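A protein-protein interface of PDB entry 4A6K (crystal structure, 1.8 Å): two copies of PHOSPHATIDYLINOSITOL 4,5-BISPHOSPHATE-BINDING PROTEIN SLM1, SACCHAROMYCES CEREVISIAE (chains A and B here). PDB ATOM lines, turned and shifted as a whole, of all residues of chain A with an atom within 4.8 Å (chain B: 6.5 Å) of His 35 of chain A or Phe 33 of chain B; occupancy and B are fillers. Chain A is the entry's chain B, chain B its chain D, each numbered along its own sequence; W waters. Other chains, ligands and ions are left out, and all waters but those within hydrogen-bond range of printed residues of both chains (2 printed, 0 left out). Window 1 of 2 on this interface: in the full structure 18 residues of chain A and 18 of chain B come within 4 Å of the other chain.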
ATOM      1  N   PHE A   4      14.844 -22.794  -4.659  1.00  0.00           N
ATOM      2  CA  PHE A   4      13.544 -23.440  -4.371  1.00  0.00           C
ATOM      3  C   PHE A   4      13.366 -23.428  -2.859  1.00  0.00           C
ATOM      4  O   PHE A   4      14.289 -23.841  -2.126  1.00  0.00           O
ATOM      5  CB  PHE A   4      13.497 -24.863  -4.997  1.00  0.00           C
ATOM      6  CG  PHE A   4      12.082 -25.407  -5.223  1.00  0.00           C
ATOM      7  CD1 PHE A   4      11.398 -26.004  -4.199  1.00  0.00           C
ATOM      8  CD2 PHE A   4      11.456 -25.341  -6.487  1.00  0.00           C
ATOM      9  CE1 PHE A   4      10.088 -26.538  -4.379  1.00  0.00           C
ATOM     10  CE2 PHE A   4      10.144 -25.835  -6.681  1.00  0.00           C
ATOM     11  CZ  PHE A   4       9.465 -26.455  -5.647  1.00  0.00           C
ATOM     12  N   TYR A  26       9.556 -38.650  -6.528  1.00  0.00           N
ATOM     13  CA  TYR A  26      10.491 -37.780  -5.826  1.00  0.00           C
ATOM     14  C   TYR A  26       9.637 -36.629  -5.225  1.00  0.00           C
ATOM     15  O   TYR A  26       9.008 -35.865  -5.953  1.00  0.00           O
ATOM     16  CB  TYR A  26      11.526 -37.149  -6.773  1.00  0.00           C
ATOM     17  CG  TYR A  26      12.562 -36.375  -6.038  1.00  0.00           C
ATOM     18  CD1 TYR A  26      13.590 -37.058  -5.300  1.00  0.00           C
ATOM     19  CD2 TYR A  26      12.539 -34.984  -5.983  1.00  0.00           C
ATOM     20  CE1 TYR A  26      14.538 -36.349  -4.571  1.00  0.00           C
ATOM     21  CE2 TYR A  26      13.508 -34.288  -5.291  1.00  0.00           C
ATOM     22  CZ  TYR A  26      14.504 -34.980  -4.565  1.00  0.00           C
ATOM     23  OH  TYR A  26      15.476 -34.366  -3.815  1.00  0.00           O
ATOM     24  N   TYR A  27       9.608 -36.537  -3.916  1.00  0.00           N
ATOM     25  CA  TYR A  27       8.686 -35.580  -3.256  1.00  0.00           C
ATOM     26  C   TYR A  27       9.428 -34.381  -2.697  1.00  0.00           C
ATOM     27  O   TYR A  27      10.595 -34.420  -2.211  1.00  0.00           O
ATOM     28  CB  TYR A  27       7.935 -36.257  -2.075  1.00  0.00           C
ATOM     29  CG  TYR A  27       6.938 -37.209  -2.573  1.00  0.00           C
ATOM     30  CD1 TYR A  27       7.319 -38.479  -2.997  1.00  0.00           C
ATOM     31  CD2 TYR A  27       5.612 -36.823  -2.676  1.00  0.00           C
ATOM     32  CE1 TYR A  27       6.343 -39.357  -3.580  1.00  0.00           C
ATOM     33  CE2 TYR A  27       4.611 -37.721  -3.171  1.00  0.00           C
ATOM     34  CZ  TYR A  27       4.997 -38.958  -3.640  1.00  0.00           C
ATOM     35  OH  TYR A  27       3.958 -39.753  -4.087  1.00  0.00           O
ATOM     36  N   VAL A  28       8.741 -33.240  -2.734  1.00  0.00           N
ATOM     37  CA  VAL A  28       9.388 -32.039  -2.221  1.00  0.00           C
ATOM     38  C   VAL A  28       8.328 -31.364  -1.381  1.00  0.00           C
ATOM     39  O   VAL A  28       7.217 -31.043  -1.858  1.00  0.00           O
ATOM     40  CB  VAL A  28       9.806 -31.080  -3.393  1.00  0.00           C
ATOM     41  CG1 VAL A  28      10.377 -29.745  -2.884  1.00  0.00           C
ATOM     42  CG2 VAL A  28      10.858 -31.793  -4.353  1.00  0.00           C
ATOM     43  N   THR A  30       7.053 -28.109   0.571  1.00  0.00           N
ATOM     44  CA  THR A  30       7.235 -26.667   0.727  1.00  0.00           C
ATOM     45  C   THR A  30       6.256 -26.252   1.832  1.00  0.00           C
ATOM     46  O   THR A  30       5.480 -27.075   2.288  1.00  0.00           O
ATOM     47  CB  THR A  30       6.896 -25.906  -0.559  1.00  0.00           C
ATOM     48  OG1 THR A  30       5.475 -25.939  -0.791  1.00  0.00           O
ATOM     49  CG2 THR A  30       7.585 -26.543  -1.743  1.00  0.00           C
ATOM     50  N   PHE A  33       2.744 -27.060  -0.028  1.00  0.00           N
ATOM     51  CA  PHE A  33       2.349 -28.274  -0.716  1.00  0.00           C
ATOM     52  C   PHE A  33       3.344 -29.412  -0.421  1.00  0.00           C
ATOM     53  O   PHE A  33       4.521 -29.162  -0.186  1.00  0.00           O
ATOM     54  CB  PHE A  33       2.465 -28.040  -2.256  1.00  0.00           C
ATOM     55  CG  PHE A  33       1.349 -27.213  -2.821  1.00  0.00           C
ATOM     56  CD1 PHE A  33       0.070 -27.775  -3.030  1.00  0.00           C
ATOM     57  CD2 PHE A  33       1.551 -25.896  -3.155  1.00  0.00           C
ATOM     58  CE1 PHE A  33      -0.967 -27.024  -3.577  1.00  0.00           C
ATOM     59  CE2 PHE A  33       0.504 -25.122  -3.697  1.00  0.00           C
ATOM     60  CZ  PHE A  33      -0.749 -25.683  -3.915  1.00  0.00           C
ATOM     61  N   LEU A  34       2.853 -30.635  -0.524  1.00  0.00           N
ATOM     62  CA  LEU A  34       3.715 -31.780  -0.778  1.00  0.00           C
ATOM     63  C   LEU A  34       3.603 -32.042  -2.286  1.00  0.00           C
ATOM     64  O   LEU A  34       2.501 -32.423  -2.813  1.00  0.00           O
ATOM     65  CB  LEU A  34       3.255 -33.026   0.048  1.00  0.00           C
ATOM     66  CG  LEU A  34       4.135 -34.282  -0.193  1.00  0.00           C
ATOM     67  CD1 LEU A  34       5.563 -34.026   0.278  1.00  0.00           C
ATOM     68  CD2 LEU A  34       3.454 -35.441   0.454  1.00  0.00           C
ATOM     69  N   HIS A  35       4.698 -31.763  -3.007  1.00  0.00           N
ATOM     70  CA  HIS A  35       4.658 -31.981  -4.469  1.00  0.00           C
ATOM     71  C   HIS A  35       5.324 -33.298  -4.782  1.00  0.00           C
ATOM     72  O   HIS A  35       6.314 -33.636  -4.152  1.00  0.00           O
ATOM     73  CB  HIS A  35       5.528 -30.928  -5.228  1.00  0.00           C
ATOM     74  CG  HIS A  35       5.104 -29.516  -5.046  1.00  0.00           C
ATOM     75  ND1 HIS A  35       3.980 -29.009  -5.634  1.00  0.00           N
ATOM     76  CD2 HIS A  35       5.688 -28.494  -4.361  1.00  0.00           C
ATOM     77  CE1 HIS A  35       3.877 -27.728  -5.309  1.00  0.00           C
ATOM     78  NE2 HIS A  35       4.917 -27.388  -4.561  1.00  0.00           N
ATOM     79  N   GLU A  36       4.773 -34.055  -5.741  1.00  0.00           N
ATOM     80  CA  GLU A  36       5.446 -35.212  -6.307  1.00  0.00           C
ATOM     81  C   GLU A  36       6.011 -34.852  -7.696  1.00  0.00           C
ATOM     82  O   GLU A  36       5.326 -34.200  -8.473  1.00  0.00           O
ATOM     83  CB  GLU A  36       4.440 -36.338  -6.454  1.00  0.00           C
ATOM     84  CG  GLU A  36       5.128 -37.670  -6.941  1.00  0.00           C
ATOM     85  CD  GLU A  36       4.079 -38.694  -7.350  1.00  0.00           C
ATOM     86  OE1 GLU A  36       2.888 -38.412  -7.175  1.00  0.00           O
ATOM     87  OE2 GLU A  36       4.473 -39.783  -7.803  1.00  0.00           O
ATOM     88  N   PHE A  37       7.235 -35.274  -8.014  1.00  0.00           N
ATOM     89  CA  PHE A  37       7.825 -35.154  -9.401  1.00  0.00           C
ATOM     90  C   PHE A  37       8.224 -36.558  -9.810  1.00  0.00           C
ATOM     91  O   PHE A  37       8.454 -37.415  -8.951  1.00  0.00           O
ATOM     92  CB  PHE A  37       9.057 -34.288  -9.417  1.00  0.00           C
ATOM     93  CG  PHE A  37       8.798 -32.910  -8.968  1.00  0.00           C
ATOM     94  CD1 PHE A  37       8.837 -32.573  -7.617  1.00  0.00           C
ATOM     95  CD2 PHE A  37       8.461 -31.949  -9.928  1.00  0.00           C
ATOM     96  CE1 PHE A  37       8.552 -31.236  -7.196  1.00  0.00           C
ATOM     97  CE2 PHE A  37       8.220 -30.626  -9.537  1.00  0.00           C
ATOM     98  CZ  PHE A  37       8.261 -30.274  -8.166  1.00  0.00           C
ATOM     99  N   LEU A  46      10.323 -30.055 -13.748  1.00  0.00           N
ATOM    100  CA  LEU A  46       9.750 -29.152 -12.786  1.00  0.00           C
ATOM    101  C   LEU A  46       8.241 -28.921 -12.887  1.00  0.00           C
ATOM    102  O   LEU A  46       7.757 -27.971 -12.293  1.00  0.00           O
ATOM    103  CB  LEU A  46      10.578 -27.847 -12.709  1.00  0.00           C
ATOM    104  CG  LEU A  46      11.857 -27.772 -11.825  1.00  0.00           C
ATOM    105  CD1 LEU A  46      12.639 -26.515 -12.088  1.00  0.00           C
ATOM    106  CD2 LEU A  46      11.618 -27.875 -10.271  1.00  0.00           C
ATOM    107  N   PRO A  48       4.974 -30.603 -11.437  1.00  0.00           N
ATOM    108  CA  PRO A  48       4.601 -31.663 -10.485  1.00  0.00           C
ATOM    109  C   PRO A  48       3.642 -32.685 -11.075  1.00  0.00           C
ATOM    110  O   PRO A  48       2.739 -32.307 -11.825  1.00  0.00           O
ATOM    111  CB  PRO A  48       3.886 -30.888  -9.331  1.00  0.00           C
ATOM    112  CG  PRO A  48       4.512 -29.530  -9.390  1.00  0.00           C
ATOM    113  CD  PRO A  48       4.710 -29.247 -10.914  1.00  0.00           C
ATOM    114  N   MET A  50       1.755 -34.196  -9.057  1.00  0.00           N
ATOM    115  CA  MET A  50       0.610 -33.749  -8.228  1.00  0.00           C
ATOM    116  C   MET A  50       1.106 -32.864  -7.120  1.00  0.00           C
ATOM    117  O   MET A  50       2.279 -32.895  -6.774  1.00  0.00           O
ATOM    118  CB  MET A  50      -0.208 -34.930  -7.672  1.00  0.00           C
ATOM    119  CG  MET A  50       0.514 -35.725  -6.571  1.00  0.00           C
ATOM    120  SD  MET A  50      -0.452 -36.979  -5.687  1.00  0.00           S
ATOM    121  CE  MET A  50       0.572 -37.054  -4.226  1.00  0.00           C
ATOM    122  N   SER A  51       0.227 -31.974  -6.633  1.00  0.00           N
ATOM    123  CA  SER A  51       0.595 -31.055  -5.560  1.00  0.00           C
ATOM    124  C   SER A  51      -0.483 -31.113  -4.509  1.00  0.00           C
ATOM    125  O   SER A  51      -1.685 -30.771  -4.796  1.00  0.00           O
ATOM    126  CB  SER A  51       0.775 -29.648  -6.127  1.00  0.00           C
ATOM    127  OG  SER A  51       1.793 -29.593  -7.182  1.00  0.00           O
ATOM    128  N   VAL B  28      -1.599 -17.506  -8.097  1.00  0.00           N
ATOM    129  CA  VAL B  28      -0.882 -17.334  -6.821  1.00  0.00           C
ATOM    130  C   VAL B  28       0.552 -17.545  -7.094  1.00  0.00           C
ATOM    131  O   VAL B  28       0.973 -18.656  -7.547  1.00  0.00           O
ATOM    132  CB  VAL B  28      -1.340 -18.437  -5.783  1.00  0.00           C
ATOM    133  CG1 VAL B  28      -0.568 -18.251  -4.447  1.00  0.00           C
ATOM    134  CG2 VAL B  28      -2.858 -18.339  -5.591  1.00  0.00           C
ATOM    135  N   LEU B  29       1.316 -16.487  -6.824  1.00  0.00           N
ATOM    136  CA  LEU B  29       2.778 -16.468  -6.998  1.00  0.00           C
ATOM    137  C   LEU B  29       3.446 -16.844  -5.676  1.00  0.00           C
ATOM    138  O   LEU B  29       3.224 -16.187  -4.685  1.00  0.00           O
ATOM    139  CB  LEU B  29       3.202 -15.052  -7.338  1.00  0.00           C
ATOM    140  CG  LEU B  29       4.688 -14.844  -7.684  1.00  0.00           C
ATOM    141  CD1 LEU B  29       5.054 -15.651  -8.915  1.00  0.00           C
ATOM    142  CD2 LEU B  29       4.850 -13.345  -7.953  1.00  0.00           C
ATOM    143  N   THR B  30       4.288 -17.854  -5.697  1.00  0.00           N
ATOM    144  CA  THR B  30       5.006 -18.234  -4.509  1.00  0.00           C
ATOM    145  C   THR B  30       6.478 -18.098  -4.891  1.00  0.00           C
ATOM    146  O   THR B  30       6.781 -17.729  -6.049  1.00  0.00           O
ATOM    147  CB  THR B  30       4.693 -19.703  -4.160  1.00  0.00           C
ATOM    148  OG1 THR B  30       5.272 -20.561  -5.163  1.00  0.00           O
ATOM    149  CG2 THR B  30       3.134 -19.923  -4.023  1.00  0.00           C
ATOM    150  N   PRO B  31       7.403 -18.326  -3.965  1.00  0.00           N
ATOM    151  CA  PRO B  31       8.822 -18.257  -4.332  1.00  0.00           C
ATOM    152  C   PRO B  31       9.203 -19.258  -5.399  1.00  0.00           C
ATOM    153  O   PRO B  31      10.167 -19.067  -6.079  1.00  0.00           O
ATOM    154  CB  PRO B  31       9.561 -18.581  -2.995  1.00  0.00           C
ATOM    155  CG  PRO B  31       8.553 -18.069  -1.959  1.00  0.00           C
ATOM    156  CD  PRO B  31       7.210 -18.540  -2.512  1.00  0.00           C
ATOM    157  N   ASN B  32       8.429 -20.343  -5.553  1.00  0.00           N
ATOM    158  CA  ASN B  32       8.726 -21.395  -6.497  1.00  0.00           C
ATOM    159  C   ASN B  32       7.903 -21.425  -7.791  1.00  0.00           C
ATOM    160  O   ASN B  32       8.380 -21.889  -8.814  1.00  0.00           O
ATOM    161  CB  ASN B  32       8.474 -22.699  -5.772  1.00  0.00           C
ATOM    162  CG  ASN B  32       9.335 -22.791  -4.473  1.00  0.00           C
ATOM    163  OD1 ASN B  32      10.472 -22.298  -4.470  1.00  0.00           O
ATOM    164  ND2 ASN B  32       8.784 -23.385  -3.390  1.00  0.00           N
ATOM    165  N   PHE B  33       6.634 -21.032  -7.732  1.00  0.00           N
ATOM    166  CA  PHE B  33       5.733 -21.238  -8.880  1.00  0.00           C
ATOM    167  C   PHE B  33       4.807 -20.083  -9.080  1.00  0.00           C
ATOM    168  O   PHE B  33       4.469 -19.314  -8.145  1.00  0.00           O
ATOM    169  CB  PHE B  33       4.781 -22.440  -8.553  1.00  0.00           C
ATOM    170  CG  PHE B  33       5.429 -23.774  -8.620  1.00  0.00           C
ATOM    171  CD1 PHE B  33       5.733 -24.347  -9.849  1.00  0.00           C
ATOM    172  CD2 PHE B  33       5.778 -24.445  -7.418  1.00  0.00           C
ATOM    173  CE1 PHE B  33       6.344 -25.578  -9.920  1.00  0.00           C
ATOM    174  CE2 PHE B  33       6.386 -25.678  -7.462  1.00  0.00           C
ATOM    175  CZ  PHE B  33       6.663 -26.275  -8.712  1.00  0.00           C
ATOM    176  N   LEU B  34       4.408 -19.913 -10.333  1.00  0.00           N
ATOM    177  CA  LEU B  34       3.159 -19.196 -10.545  1.00  0.00           C
ATOM    178  C   LEU B  34       2.076 -20.295 -10.731  1.00  0.00           C
ATOM    179  O   LEU B  34       2.065 -21.051 -11.733  1.00  0.00           O
ATOM    180  CB  LEU B  34       3.301 -18.253 -11.768  1.00  0.00           C
ATOM    181  CG  LEU B  34       2.011 -17.480 -12.114  1.00  0.00           C
ATOM    182  CD1 LEU B  34       1.613 -16.444 -11.054  1.00  0.00           C
ATOM    183  CD2 LEU B  34       2.239 -16.818 -13.504  1.00  0.00           C
ATOM    184  N   HIS B  35       1.187 -20.438  -9.737  1.00  0.00           N
ATOM    185  CA  HIS B  35       0.067 -21.425  -9.819  1.00  0.00           C
ATOM    186  C   HIS B  35      -1.176 -20.750 -10.358  1.00  0.00           C
ATOM    187  O   HIS B  35      -1.437 -19.589 -10.003  1.00  0.00           O
ATOM    188  CB  HIS B  35      -0.331 -21.950  -8.383  1.00  0.00           C
ATOM    189  CG  HIS B  35       0.798 -22.619  -7.637  1.00  0.00           C
ATOM    190  ND1 HIS B  35       1.284 -23.851  -7.977  1.00  0.00           N
ATOM    191  CD2 HIS B  35       1.518 -22.210  -6.560  1.00  0.00           C
ATOM    192  CE1 HIS B  35       2.254 -24.186  -7.142  1.00  0.00           C
ATOM    193  NE2 HIS B  35       2.384 -23.232  -6.252  1.00  0.00           N
ATOM    194  N   PRO B  48      -4.025 -26.865  -8.227  1.00  0.00           N
ATOM    195  CA  PRO B  48      -3.671 -25.966  -9.318  1.00  0.00           C
ATOM    196  C   PRO B  48      -4.069 -26.575 -10.653  1.00  0.00           C
ATOM    197  O   PRO B  48      -3.892 -27.817 -10.900  1.00  0.00           O
ATOM    198  CB  PRO B  48      -2.134 -25.857  -9.218  1.00  0.00           C
ATOM    199  CG  PRO B  48      -1.863 -26.038  -7.734  1.00  0.00           C
ATOM    200  CD  PRO B  48      -2.837 -27.206  -7.421  1.00  0.00           C
ATOM    201  N   SER B  51       1.027 -25.387 -12.559  1.00  0.00           N
ATOM    202  CA  SER B  51       2.020 -24.709 -11.761  1.00  0.00           C
ATOM    203  C   SER B  51       3.246 -24.467 -12.611  1.00  0.00           C
ATOM    204  O   SER B  51       3.931 -25.439 -12.992  1.00  0.00           O
ATOM    205  CB  SER B  51       2.393 -25.596 -10.553  1.00  0.00           C
ATOM    206  OG  SER B  51       1.246 -25.877  -9.726  1.00  0.00           O
ATOM    207  N   LEU B  52       3.561 -23.197 -12.886  1.00  0.00           N
ATOM    208  CA  LEU B  52       4.693 -22.828 -13.728  1.00  0.00           C
ATOM    209  C   LEU B  52       5.918 -22.604 -12.868  1.00  0.00           C
ATOM    210  O   LEU B  52       5.984 -21.690 -12.068  1.00  0.00           O
ATOM    211  CB  LEU B  52       4.357 -21.500 -14.448  1.00  0.00           C
ATOM    212  CG  LEU B  52       3.242 -21.546 -15.494  1.00  0.00           C
ATOM    213  CD1 LEU B  52       2.793 -20.083 -15.835  1.00  0.00           C
ATOM    214  CD2 LEU B  52       3.746 -22.228 -16.768  1.00  0.00           C
ATOM    215  N   ALA B  53       6.950 -23.407 -13.051  1.00  0.00           N
ATOM    216  CA  ALA B  53       8.167 -23.202 -12.241  1.00  0.00           C
ATOM    217  C   ALA B  53       8.941 -21.946 -12.614  1.00  0.00           C
ATOM    218  O   ALA B  53       9.326 -21.778 -13.743  1.00  0.00           O
ATOM    219  CB  ALA B  53       9.125 -24.455 -12.352  1.00  0.00           C
ATOM    220  N   LEU B  54       9.164 -21.095 -11.641  1.00  0.00           N
ATOM    221  CA  LEU B  54       9.756 -19.774 -11.909  1.00  0.00           C
ATOM    222  C   LEU B  54      11.222 -19.901 -12.378  1.00  0.00           C
ATOM    223  O   LEU B  54      11.686 -19.083 -13.226  1.00  0.00           O
ATOM    224  CB  LEU B  54       9.674 -18.891 -10.698  1.00  0.00           C
ATOM    225  CG  LEU B  54       8.252 -18.574 -10.220  1.00  0.00           C
ATOM    226  CD1 LEU B  54       8.352 -17.708  -8.997  1.00  0.00           C
ATOM    227  CD2 LEU B  54       7.362 -17.907 -11.310  1.00  0.00           C
HETATM  228  O   HOH W   1       0.802 -28.582  -9.506  1.00  0.00           O
HETATM  229  O   HOH W   2       6.353 -26.153 -14.127  1.00  0.00           O
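OG1 of Thr 30 of chain A sits at hydrogen-bond distance from N of Phe 33 of chain A (3.0 Å).
The side-chain hydroxyl of Ser 51 of chain A sits at hydrogen-bond distance from a ring nitrogen (ND1) of His 35 of chain A (2.7 Å).
The backbone NH (N) of Val 28 of chain B lies within hydrogen-bond range of the backbone carbonyl oxygen (O) of His 35 of chain B, 2.8 Å away.
N of Asn 32 of chain B sits close to OG1 of Thr 30 of chain B (3.2 Å).
The side-chain hydroxyl (OG1) of Thr 30 of chain B lies within hydrogen-bond range of the backbone NH (N) of Phe 33 of chain B (2.9 Å).
The backbone carbonyl oxygen of Asn 32 of chain B lies within hydrogen-bond range of the backbone NH of Leu 54 of chain B (3.0 Å).
Of the 13 printed residues of chain B, 5 touch a printed residue of chain A.
Hydrophobic or aromatic side chains of chain B that line the printed part of chain A: Phe 33, His 35, Pro 48 and Ala 53.
Of the 14 printed residues of chain A, 6 touch a printed residue of chain B.
Hydrophobic or aromatic side chains of chain A that line the printed part of chain B: Phe 4, Phe 33, His 35, Leu 46 and Pro 48.
Among the printed residues, 9 pairs touch across the chains.
Among the printed residues, no Asp or Glu carboxylate lies within 4 Å of a Lys or Arg side-chain nitrogen of the other chain.
OD1 of Asn 32 of chain B touches CA of Phe 4 of chain A, 3.3 Å away.
Phe 4 of chain A touches Phe 33 of chain B (CZ to CE2, 3.7 Å).
Thr 30 of chain A touches Asn 32 of chain B.
His 35 of chain B touches Phe 33 of chain A.
Phe 33 of chain A touches Pro 48 of chain B.
His 35 of chain A touches Phe 33 of chain B (NE2 to CE2, 3.7 Å).
O of Leu 46 of chain A touches CE1 of Phe 33 of chain B, 3.7 Å away.
Ala 53 of chain B touches Leu 46 of chain A (CB to CB, 3.7 Å).
Pro 48 of chain A touches Phe 33 of chain B.
Water W1 bridges OG of Ser 51 of chain A (2.7 Å) and OG of Ser 51 of chain B (2.8 Å).
Water W2 lies within hydrogen-bond range of O of Ser 51 of chain B, O of Leu 46 of chain A and N of Ala 53 of chain B.
His 35 of chain A touches one residue of chain B.
Of the printed residues of chain A, Phe 33 of chain B touches Phe 4 (3.7 Å), His 35 (3.7 Å), Leu 46 (3.7 Å) and Pro 48 (3.96 Å).
Printed residues of chain A within 4 Å of Pro 48 of chain B: Phe 33.
Of the printed residues of chain B, Pro 48 of chain A touches Phe 33 (3.96 Å).
Printed residues of chain B within 4 Å of Phe 33 of chain A: His 35 and Pro 48.
Glu 36 of chain A touches none of the printed residues of chain B.
The nearest residue of chain A that does not touch Phe 33 of chain B is Phe 37 of chain A (4.3 Å).
The nearest printed residue of chain B that does not touch Phe 4 of chain A is Pro 31 of chain B (5.8 Å).
Phe 33 of chain A touches His 35 of chain B, and with the chains exchanged His 35 of chain A touches Phe 33 of chain B.
Phe 33 of chain A touches Pro 48 of chain B, and with the chains exchanged Pro 48 of chain A touches Phe 33 of chain B.
Positions printed for both chains: 28, 30, 33, 34, 35, 48 and 51.
Of the 9 pairs that touch across the chains among the printed residues, 4 have their exchanged pair printed and touching as well.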
